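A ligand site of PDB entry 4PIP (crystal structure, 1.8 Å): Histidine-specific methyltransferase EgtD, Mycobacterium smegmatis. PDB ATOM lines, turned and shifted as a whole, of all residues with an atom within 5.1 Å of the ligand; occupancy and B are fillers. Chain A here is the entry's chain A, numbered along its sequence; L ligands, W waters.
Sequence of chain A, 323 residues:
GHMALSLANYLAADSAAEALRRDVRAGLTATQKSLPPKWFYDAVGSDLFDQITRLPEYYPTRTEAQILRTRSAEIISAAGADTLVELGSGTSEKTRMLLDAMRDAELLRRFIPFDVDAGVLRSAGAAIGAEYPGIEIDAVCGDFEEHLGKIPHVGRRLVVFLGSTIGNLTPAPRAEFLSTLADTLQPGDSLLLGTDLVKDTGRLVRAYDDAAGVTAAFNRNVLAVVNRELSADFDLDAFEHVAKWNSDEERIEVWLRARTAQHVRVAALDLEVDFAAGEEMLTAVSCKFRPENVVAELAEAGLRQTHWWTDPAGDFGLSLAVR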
ATOM      1  N   LYS A  38      11.885  -8.214 -25.459  1.00  0.00           N
ATOM      2  CA  LYS A  38      10.795  -7.484 -24.806  1.00  0.00           C
ATOM      3  C   LYS A  38      11.338  -6.353 -23.912  1.00  0.00           C
ATOM      4  O   LYS A  38      10.638  -5.386 -23.611  1.00  0.00           O
ATOM      5  CB  LYS A  38       9.907  -8.433 -24.003  1.00  0.00           C
ATOM      6  CG  LYS A  38      10.588  -9.233 -22.913  1.00  0.00           C
ATOM      7  CD  LYS A  38       9.615 -10.208 -22.220  1.00  0.00           C
ATOM      8  CE  LYS A  38       9.631 -11.600 -22.863  1.00  0.00           C
ATOM      9  NZ  LYS A  38       8.670 -12.567 -22.246  1.00  0.00           N
ATOM     10  N   TYR A  41      12.431  -1.875 -24.780  1.00  0.00           N
ATOM     11  CA  TYR A  41      11.613  -0.684 -24.963  1.00  0.00           C
ATOM     12  C   TYR A  41      11.318   0.140 -23.698  1.00  0.00           C
ATOM     13  O   TYR A  41      10.171   0.532 -23.477  1.00  0.00           O
ATOM     14  CB  TYR A  41      10.285  -1.074 -25.618  1.00  0.00           C
ATOM     15  CG  TYR A  41      10.471  -1.933 -26.855  1.00  0.00           C
ATOM     16  CD1 TYR A  41      10.650  -3.314 -26.757  1.00  0.00           C
ATOM     17  CD2 TYR A  41      10.488  -1.358 -28.118  1.00  0.00           C
ATOM     18  CE1 TYR A  41      10.816  -4.086 -27.919  1.00  0.00           C
ATOM     19  CE2 TYR A  41      10.664  -2.111 -29.252  1.00  0.00           C
ATOM     20  CZ  TYR A  41      10.828  -3.464 -29.156  1.00  0.00           C
ATOM     21  OH  TYR A  41      10.984  -4.178 -30.340  1.00  0.00           O
ATOM     22  N   SER A  46      12.416   3.058 -26.457  1.00  0.00           N
ATOM     23  CA  SER A  46      11.188   3.354 -27.199  1.00  0.00           C
ATOM     24  C   SER A  46      11.384   4.563 -28.100  1.00  0.00           C
ATOM     25  O   SER A  46      10.866   4.633 -29.218  1.00  0.00           O
ATOM     26  CB  SER A  46      10.017   3.585 -26.247  1.00  0.00           C
ATOM     27  OG  SER A  46       9.614   2.380 -25.638  1.00  0.00           O
ATOM     28  N   PHE A  49      13.374   3.367 -30.974  1.00  0.00           N
ATOM     29  CA  PHE A  49      12.488   2.603 -31.892  1.00  0.00           C
ATOM     30  C   PHE A  49      11.713   3.583 -32.752  1.00  0.00           C
ATOM     31  O   PHE A  49      11.687   3.452 -33.907  1.00  0.00           O
ATOM     32  CB  PHE A  49      11.494   1.725 -31.205  1.00  0.00           C
ATOM     33  CG  PHE A  49      10.689   0.909 -32.172  1.00  0.00           C
ATOM     34  CD1 PHE A  49      11.226  -0.133 -32.749  1.00  0.00           C
ATOM     35  CD2 PHE A  49       9.462   1.268 -32.523  1.00  0.00           C
ATOM     36  CE1 PHE A  49      10.535  -0.890 -33.675  1.00  0.00           C
ATOM     37  CE2 PHE A  49       8.731   0.540 -33.447  1.00  0.00           C
ATOM     38  CZ  PHE A  49       9.291  -0.541 -34.028  1.00  0.00           C
ATOM     39  N   THR A  61       7.397  -0.040 -40.818  1.00  0.00           N
ATOM     40  CA  THR A  61       6.381   0.802 -40.174  1.00  0.00           C
ATOM     41  C   THR A  61       5.517   1.568 -41.168  1.00  0.00           C
ATOM     42  O   THR A  61       4.276   1.542 -41.112  1.00  0.00           O
ATOM     43  CB  THR A  61       7.003   1.833 -39.216  1.00  0.00           C
ATOM     44  OG1 THR A  61       7.805   1.172 -38.240  1.00  0.00           O
ATOM     45  CG2 THR A  61       5.920   2.626 -38.518  1.00  0.00           C
ATOM     46  N   GLU A  64       3.284  -0.845 -43.299  1.00  0.00           N
ATOM     47  CA  GLU A  64       2.071  -1.233 -42.603  1.00  0.00           C
ATOM     48  C   GLU A  64       1.145  -0.031 -42.405  1.00  0.00           C
ATOM     49  O   GLU A  64      -0.076  -0.182 -42.453  1.00  0.00           O
ATOM     50  CB  GLU A  64       2.398  -1.887 -41.260  1.00  0.00           C
ATOM     51  CG  GLU A  64       1.171  -2.359 -40.464  1.00  0.00           C
ATOM     52  CD  GLU A  64       1.573  -3.132 -39.225  1.00  0.00           C
ATOM     53  OE1 GLU A  64       2.459  -2.651 -38.482  1.00  0.00           O
ATOM     54  OE2 GLU A  64       1.021  -4.226 -39.016  1.00  0.00           O
ATOM     55  N   GLU A  86      -4.824  -3.079 -28.164  1.00  0.00           N
ATOM     56  CA  GLU A  86      -3.562  -3.107 -28.902  1.00  0.00           C
ATOM     57  C   GLU A  86      -2.506  -3.807 -28.099  1.00  0.00           C
ATOM     58  O   GLU A  86      -2.125  -3.367 -27.002  1.00  0.00           O
ATOM     59  CB  GLU A  86      -3.070  -1.717 -29.280  1.00  0.00           C
ATOM     60  CG  GLU A  86      -1.769  -1.824 -30.101  1.00  0.00           C
ATOM     61  CD  GLU A  86      -1.482  -0.617 -30.957  1.00  0.00           C
ATOM     62  OE1 GLU A  86      -1.877   0.514 -30.569  1.00  0.00           O
ATOM     63  OE2 GLU A  86      -0.839  -0.806 -32.033  1.00  0.00           O
ATOM     64  N   LEU A  87      -1.985  -4.878 -28.692  1.00  0.00           N
ATOM     65  CA  LEU A  87      -0.889  -5.611 -28.084  1.00  0.00           C
ATOM     66  C   LEU A  87       0.435  -5.002 -28.501  1.00  0.00           C
ATOM     67  O   LEU A  87       0.812  -5.066 -29.676  1.00  0.00           O
ATOM     68  CB  LEU A  87      -0.936  -7.077 -28.469  1.00  0.00           C
ATOM     69  CG  LEU A  87      -2.217  -7.831 -28.145  1.00  0.00           C
ATOM     70  CD1 LEU A  87      -2.072  -9.259 -28.625  1.00  0.00           C
ATOM     71  CD2 LEU A  87      -2.518  -7.787 -26.630  1.00  0.00           C
ATOM     72  N   GLY A  88       1.155  -4.435 -27.536  1.00  0.00           N
ATOM     73  CA  GLY A  88       2.352  -3.681 -27.838  1.00  0.00           C
ATOM     74  C   GLY A  88       1.948  -2.296 -28.341  1.00  0.00           C
ATOM     75  O   GLY A  88       1.483  -2.159 -29.458  1.00  0.00           O
ATOM     76  N   SER A  89       2.134  -1.286 -27.486  1.00  0.00           N
ATOM     77  CA  SER A  89       1.742   0.083 -27.828  1.00  0.00           C
ATOM     78  C   SER A  89       2.954   0.812 -28.356  1.00  0.00           C
ATOM     79  O   SER A  89       3.830   0.185 -28.956  1.00  0.00           O
ATOM     80  CB  SER A  89       1.165   0.779 -26.601  1.00  0.00           C
ATOM     81  OG  SER A  89       0.207  -0.057 -25.973  1.00  0.00           O
ATOM     82  N   GLY A  90       3.004   2.134 -28.171  1.00  0.00           N
ATOM     83  CA  GLY A  90       4.210   2.891 -28.450  1.00  0.00           C
ATOM     84  C   GLY A  90       4.340   3.541 -29.819  1.00  0.00           C
ATOM     85  O   GLY A  90       5.277   4.316 -30.030  1.00  0.00           O
ATOM     86  N   THR A  91       3.424   3.245 -30.739  1.00  0.00           N
ATOM     87  CA  THR A  91       3.479   3.823 -32.092  1.00  0.00           C
ATOM     88  C   THR A  91       2.086   4.291 -32.489  1.00  0.00           C
ATOM     89  O   THR A  91       1.393   3.664 -33.297  1.00  0.00           O
ATOM     90  CB  THR A  91       4.016   2.801 -33.121  1.00  0.00           C
ATOM     91  OG1 THR A  91       5.306   2.349 -32.700  1.00  0.00           O
ATOM     92  CG2 THR A  91       4.151   3.426 -34.523  1.00  0.00           C
ATOM     93  N   LYS A  94      -0.312   4.486 -35.941  1.00  0.00           N
ATOM     94  CA  LYS A  94      -1.111   3.384 -36.474  1.00  0.00           C
ATOM     95  C   LYS A  94      -2.388   3.214 -35.662  1.00  0.00           C
ATOM     96  O   LYS A  94      -3.433   2.906 -36.220  1.00  0.00           O
ATOM     97  CB  LYS A  94      -0.293   2.093 -36.496  1.00  0.00           C
ATOM     98  CG  LYS A  94       0.844   2.165 -37.505  1.00  0.00           C
ATOM     99  CD  LYS A  94       1.533   0.820 -37.801  1.00  0.00           C
ATOM    100  CE  LYS A  94       2.410   0.372 -36.650  1.00  0.00           C
ATOM    101  NZ  LYS A  94       3.384  -0.674 -37.074  1.00  0.00           N
ATOM    102  N   PHE A 114      -2.031  -2.479 -24.318  1.00  0.00           N
ATOM    103  CA  PHE A 114      -1.379  -3.553 -23.587  1.00  0.00           C
ATOM    104  C   PHE A 114       0.134  -3.517 -23.839  1.00  0.00           C
ATOM    105  O   PHE A 114       0.557  -3.623 -24.977  1.00  0.00           O
ATOM    106  CB  PHE A 114      -1.960  -4.878 -24.012  1.00  0.00           C
ATOM    107  CG  PHE A 114      -1.375  -6.074 -23.300  1.00  0.00           C
ATOM    108  CD1 PHE A 114      -0.146  -6.575 -23.638  1.00  0.00           C
ATOM    109  CD2 PHE A 114      -2.101  -6.723 -22.319  1.00  0.00           C
ATOM    110  CE1 PHE A 114       0.380  -7.685 -22.991  1.00  0.00           C
ATOM    111  CE2 PHE A 114      -1.577  -7.830 -21.663  1.00  0.00           C
ATOM    112  CZ  PHE A 114      -0.340  -8.304 -22.008  1.00  0.00           C
ATOM    113  N   ASP A 115       0.946  -3.370 -22.797  1.00  0.00           N
ATOM    114  CA  ASP A 115       2.400  -3.281 -22.973  1.00  0.00           C
ATOM    115  C   ASP A 115       3.140  -3.759 -21.749  1.00  0.00           C
ATOM    116  O   ASP A 115       2.619  -3.661 -20.643  1.00  0.00           O
ATOM    117  CB  ASP A 115       2.801  -1.841 -23.293  1.00  0.00           C
ATOM    118  CG  ASP A 115       4.061  -1.757 -24.134  1.00  0.00           C
ATOM    119  OD1 ASP A 115       5.153  -1.927 -23.566  1.00  0.00           O
ATOM    120  OD2 ASP A 115       3.952  -1.562 -25.366  1.00  0.00           O
ATOM    121  N   VAL A 116       4.377  -4.227 -21.922  1.00  0.00           N
ATOM    122  CA  VAL A 116       5.145  -4.687 -20.772  1.00  0.00           C
ATOM    123  C   VAL A 116       5.793  -3.502 -20.045  1.00  0.00           C
ATOM    124  O   VAL A 116       6.242  -3.635 -18.901  1.00  0.00           O
ATOM    125  CB  VAL A 116       6.215  -5.718 -21.199  1.00  0.00           C
ATOM    126  CG1 VAL A 116       7.313  -5.063 -22.034  1.00  0.00           C
ATOM    127  CG2 VAL A 116       6.805  -6.415 -19.971  1.00  0.00           C
ATOM    128  N   ASP A 117       5.793  -2.341 -20.685  1.00  0.00           N
ATOM    129  CA  ASP A 117       6.400  -1.152 -20.110  1.00  0.00           C
ATOM    130  C   ASP A 117       5.325  -0.176 -19.634  1.00  0.00           C
ATOM    131  O   ASP A 117       4.530   0.318 -20.422  1.00  0.00           O
ATOM    132  CB  ASP A 117       7.318  -0.469 -21.141  1.00  0.00           C
ATOM    133  CG  ASP A 117       8.227   0.555 -20.511  1.00  0.00           C
ATOM    134  OD1 ASP A 117       7.787   1.704 -20.347  1.00  0.00           O
ATOM    135  OD2 ASP A 117       9.390   0.209 -20.212  1.00  0.00           O
ATOM    136  N   VAL A 120       5.266   3.477 -21.390  1.00  0.00           N
ATOM    137  CA  VAL A 120       4.627   3.533 -22.707  1.00  0.00           C
ATOM    138  C   VAL A 120       3.106   3.583 -22.604  1.00  0.00           C
ATOM    139  O   VAL A 120       2.449   4.331 -23.335  1.00  0.00           O
ATOM    140  CB  VAL A 120       5.077   2.331 -23.566  1.00  0.00           C
ATOM    141  CG1 VAL A 120       4.317   2.259 -24.903  1.00  0.00           C
ATOM    142  CG2 VAL A 120       6.613   2.403 -23.771  1.00  0.00           C
ATOM    143  N   GLY A 142       1.622  -5.875 -18.845  1.00  0.00           N
ATOM    144  CA  GLY A 142       1.930  -7.286 -18.856  1.00  0.00           C
ATOM    145  C   GLY A 142       2.730  -7.709 -20.086  1.00  0.00           C
ATOM    146  O   GLY A 142       3.008  -6.901 -20.961  1.00  0.00           O
ATOM    147  N   ASP A 143       3.086  -8.987 -20.087  1.00  0.00           N
ATOM    148  CA  ASP A 143       3.794  -9.682 -21.151  1.00  0.00           C
ATOM    149  C   ASP A 143       2.756 -10.410 -22.000  1.00  0.00           C
ATOM    150  O   ASP A 143       1.981 -11.194 -21.452  1.00  0.00           O
ATOM    151  CB  ASP A 143       4.778 -10.661 -20.510  1.00  0.00           C
ATOM    152  CG  ASP A 143       5.608 -11.435 -21.495  1.00  0.00           C
ATOM    153  OD1 ASP A 143       5.285 -11.452 -22.687  1.00  0.00           O
ATOM    154  OD2 ASP A 143       6.598 -12.052 -21.040  1.00  0.00           O
ATOM    155  N   PHE A 144       2.732 -10.194 -23.315  1.00  0.00           N
ATOM    156  CA  PHE A 144       1.672 -10.810 -24.109  1.00  0.00           C
ATOM    157  C   PHE A 144       1.900 -12.308 -24.285  1.00  0.00           C
ATOM    158  O   PHE A 144       1.067 -12.974 -24.854  1.00  0.00           O
ATOM    159  CB  PHE A 144       1.483 -10.130 -25.481  1.00  0.00           C
ATOM    160  CG  PHE A 144       2.764  -9.928 -26.281  1.00  0.00           C
ATOM    161  CD1 PHE A 144       3.541 -10.998 -26.680  1.00  0.00           C
ATOM    162  CD2 PHE A 144       3.121  -8.661 -26.705  1.00  0.00           C
ATOM    163  CE1 PHE A 144       4.691 -10.795 -27.427  1.00  0.00           C
ATOM    164  CE2 PHE A 144       4.259  -8.458 -27.466  1.00  0.00           C
ATOM    165  CZ  PHE A 144       5.041  -9.519 -27.824  1.00  0.00           C
ATOM    166  N   GLU A 145       3.018 -12.834 -23.764  1.00  0.00           N
ATOM    167  CA  GLU A 145       3.191 -14.279 -23.689  1.00  0.00           C
ATOM    168  C   GLU A 145       2.657 -14.907 -22.396  1.00  0.00           C
ATOM    169  O   GLU A 145       2.626 -16.128 -22.285  1.00  0.00           O
ATOM    170  CB  GLU A 145       4.680 -14.650 -23.799  1.00  0.00           C
ATOM    171  CG  GLU A 145       5.297 -14.339 -25.127  1.00  0.00           C
ATOM    172  CD  GLU A 145       6.695 -14.908 -25.258  1.00  0.00           C
ATOM    173  OE1 GLU A 145       7.667 -14.152 -25.032  1.00  0.00           O
ATOM    174  OE2 GLU A 145       6.825 -16.107 -25.581  1.00  0.00           O
ATOM    175  N   LEU A 162       0.437  -5.294 -34.215  1.00  0.00           N
ATOM    176  CA  LEU A 162       1.053  -4.754 -35.425  1.00  0.00           C
ATOM    177  C   LEU A 162       2.578  -4.728 -35.345  1.00  0.00           C
ATOM    178  O   LEU A 162       3.171  -5.115 -34.330  1.00  0.00           O
ATOM    179  CB  LEU A 162       0.535  -3.338 -35.674  1.00  0.00           C
ATOM    180  CG  LEU A 162      -0.996  -3.210 -35.579  1.00  0.00           C
ATOM    181  CD1 LEU A 162      -1.422  -1.761 -35.739  1.00  0.00           C
ATOM    182  CD2 LEU A 162      -1.647  -4.084 -36.640  1.00  0.00           C
ATOM    183  N   GLY A 163       3.205  -4.296 -36.430  1.00  0.00           N
ATOM    184  CA  GLY A 163       4.642  -4.032 -36.452  1.00  0.00           C
ATOM    185  C   GLY A 163       5.494  -5.267 -36.658  1.00  0.00           C
ATOM    186  O   GLY A 163       6.732  -5.229 -36.557  1.00  0.00           O
ATOM    187  N   THR A 165       5.600  -7.579 -34.649  1.00  0.00           N
ATOM    188  CA  THR A 165       6.059  -7.924 -33.312  1.00  0.00           C
ATOM    189  C   THR A 165       5.914  -9.434 -33.100  1.00  0.00           C
ATOM    190  O   THR A 165       6.726 -10.046 -32.398  1.00  0.00           O
ATOM    191  CB  THR A 165       5.271  -7.135 -32.213  1.00  0.00           C
ATOM    192  OG1 THR A 165       5.419  -5.729 -32.411  1.00  0.00           O
ATOM    193  CG2 THR A 165       5.765  -7.485 -30.822  1.00  0.00           C
HETATM  194  N1  LIG L   1       2.668  -1.563 -31.976  1.00  0.00           N
HETATM  195  C1  LIG L   1       3.940  -0.920 -32.233  1.00  0.00           C
HETATM  196  C2  LIG L   1       5.052  -1.758 -31.629  1.00  0.00           C
HETATM  197  C3  LIG L   1       6.111  -0.845 -31.043  1.00  0.00           C
HETATM  198  S1  LIG L   1       7.626  -1.701 -30.615  1.00  0.00           S
HETATM  199  C4  LIG L   1       4.221  -0.812 -33.717  1.00  0.00           C
HETATM  200  O1  LIG L   1       5.107  -0.051 -34.132  1.00  0.00           O
HETATM  201  O2  LIG L   1       3.579  -1.488 -34.506  1.00  0.00           O
HETATM  202  C5  LIG L   1       6.894  -2.981 -29.542  1.00  0.00           C
HETATM  203  C6  LIG L   1       6.091  -2.512 -28.318  1.00  0.00           C
HETATM  204  O3  LIG L   1       5.580  -3.690 -27.734  1.00  0.00           O
HETATM  205  C7  LIG L   1       6.898  -1.788 -27.232  1.00  0.00           C
HETATM  206  O4  LIG L   1       6.151  -0.792 -26.583  1.00  0.00           O
HETATM  207  C8  LIG L   1       7.228  -2.870 -26.243  1.00  0.00           C
HETATM  208  O5  LIG L   1       7.396  -2.403 -24.916  1.00  0.00           O
HETATM  209  C9  LIG L   1       6.057  -3.825 -26.420  1.00  0.00           C
HETATM  210  N2  LIG L   1       6.426  -5.224 -26.192  1.00  0.00           N
HETATM  211  C10 LIG L   1       7.482  -5.906 -26.729  1.00  0.00           C
HETATM  212  N3  LIG L   1       7.456  -7.168 -26.245  1.00  0.00           N
HETATM  213  C11 LIG L   1       6.402  -7.286 -25.406  1.00  0.00           C
HETATM  214  C12 LIG L   1       5.898  -8.332 -24.659  1.00  0.00           C
HETATM  215  N4  LIG L   1       6.491  -9.517 -24.664  1.00  0.00           N
HETATM  216  N5  LIG L   1       4.779  -8.135 -23.888  1.00  0.00           N
HETATM  217  C13 LIG L   1       4.139  -6.910 -23.875  1.00  0.00           C
HETATM  218  N6  LIG L   1       4.634  -5.869 -24.622  1.00  0.00           N
HETATM  219  C14 LIG L   1       5.741  -6.065 -25.375  1.00  0.00           C
HETATM  220  O   HOH W   1       7.335   1.652 -26.949  1.00  0.00           O
HETATM  221  O   HOH W   2       6.185  -0.393 -36.718  1.00  0.00           O
HETATM  222  O   HOH W   3       8.311 -11.391 -26.203  1.00  0.00           O
HETATM  223  O   HOH W   4       3.148  -4.476 -31.482  1.00  0.00           O
HETATM  224  O   HOH W   5       9.884  -2.922 -23.133  1.00  0.00           O
HETATM  225  O   HOH W   6       8.432   1.358 -29.352  1.00  0.00           O
HETATM  226  O   HOH W   7       1.008   0.517 -32.950  1.00  0.00           O
HETATM  227  O   HOH W   8       8.006  -4.441 -32.427  1.00  0.00           O
HETATM  228  O   HOH W   9       9.398  -8.441 -27.999  1.00  0.00           O
HETATM  229  O   HOH W  10       0.141  -3.435 -32.107  1.00  0.00           O
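The backbone carbonyl oxygen (O) of Gly 88 is in hydrogen-bond range of a nitrogen (N1) of the ligand, 2.8 Å away.
OG1 of Thr 91 lies within hydrogen-bond range of O1 of the ligand, at 2.8 Å.
O2 of the ligand lies within salt-bridge range of NZ of Lys 94 (2.7 Å).
OD1 of Asp 143 sits at hydrogen-bond distance from N4 of the ligand (3.0 Å).
The backbone carbonyl oxygen of Ser 89 lies close to an oxygen (O4) of the ligand (3.5 Å).
A nitrogen (N6) of the ligand is in hydrogen-bond range of the backbone NH of Val 116 (3.2 Å).
OD2 of Asp 115 is in hydrogen-bond range of O4 of the ligand.
OE2 of Glu 86 is in salt-bridge range of N1 of the ligand (3.6 Å).
The backbone NH (N) of Phe 144 lies within hydrogen-bond range of a nitrogen (N5) of the ligand (3.0 Å).
An oxygen (O2) of the ligand sits close to the backbone NH of Gly 163, 3.4 Å away.
The backbone NH (N) of Gly 88 sits at hydrogen-bond distance from the backbone carbonyl oxygen (O) of Phe 114 (2.8 Å).
NZ of Lys 94 is in salt-bridge range of OE1 of Glu 64, at 2.6 Å.
The backbone carbonyl oxygen (O) of Tyr 41 is in hydrogen-bond range of the side-chain hydroxyl (OG) of Ser 46 (2.9 Å).
O of Gly 142 sits close to N of Val 116, 3.2 Å away.
The side-chain amino group (NZ) of Lys 38 is in salt-bridge range of the side-chain carboxylate (OE1) of Glu 145, at 3.4 Å.
N of Gly 142 sits at hydrogen-bond distance from O of Asp 115.
N of Val 120 is in hydrogen-bond range of OD1 of Asp 117, 3.3 Å away.
N of Phe 114 is in hydrogen-bond range of O of Glu 86.
Lys 38 touches the ligand (CB to N3, 3.6 Å).
Tyr 41 touches the ligand.
Phe 49 touches the ligand.
Phe 114 touches the ligand.
CG1 of Val 120 touches O4 of the ligand, at 3.9 Å.
O of Gly 142 touches C13 of the ligand (3.1 Å).
Leu 162 touches the ligand (C to O2, 3.5 Å).
Hydrophobic or aromatic side chains that line the ligand: Tyr 41, Phe 49, Phe 114, Val 116, Val 120, Phe 144 and Leu 162.
17 residues have an atom within 4 Å of the ligand: Lys 38, Tyr 41, Phe 49, Glu 86, Gly 88, Ser 89, Thr 91, Lys 94, Phe 114, Asp 115, Val 116, Val 120, Gly 142, Asp 143, Phe 144, Leu 162 and Gly 163.
The nearest printed residue that does not touch the ligand is Thr 165 (4.1 Å).
Water W1 bridges the side-chain hydroxyl of Ser 46 (2.7 Å) and an oxygen (O4) of the ligand (2.7 Å).
Water W2 lies within hydrogen-bond range of the side-chain hydroxyl (OG1) of Thr 61 (2.7 Å), an oxygen (O1) of the ligand (2.8 Å) and the side-chain amino group (NZ) of Lys 94 (2.8 Å).
Water W7 lies within hydrogen-bond range of OE2 of Glu 86 (2.5 Å), N1 of the ligand (2.8 Å) and O of Thr 91 (3.2 Å).
Water W3 lies within hydrogen-bond range of N4 of the ligand (3.0 Å) and OE1 of Glu 145 (3.1 Å).
Water W5 lies within hydrogen-bond range of the backbone carbonyl oxygen (O) of Lys 38, an oxygen (O5) of the ligand and the backbone NH (N) of Tyr 41.
Water W8 bridges OG1 of Thr 165 (2.9 Å) and S1 of the ligand (3.3 Å).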
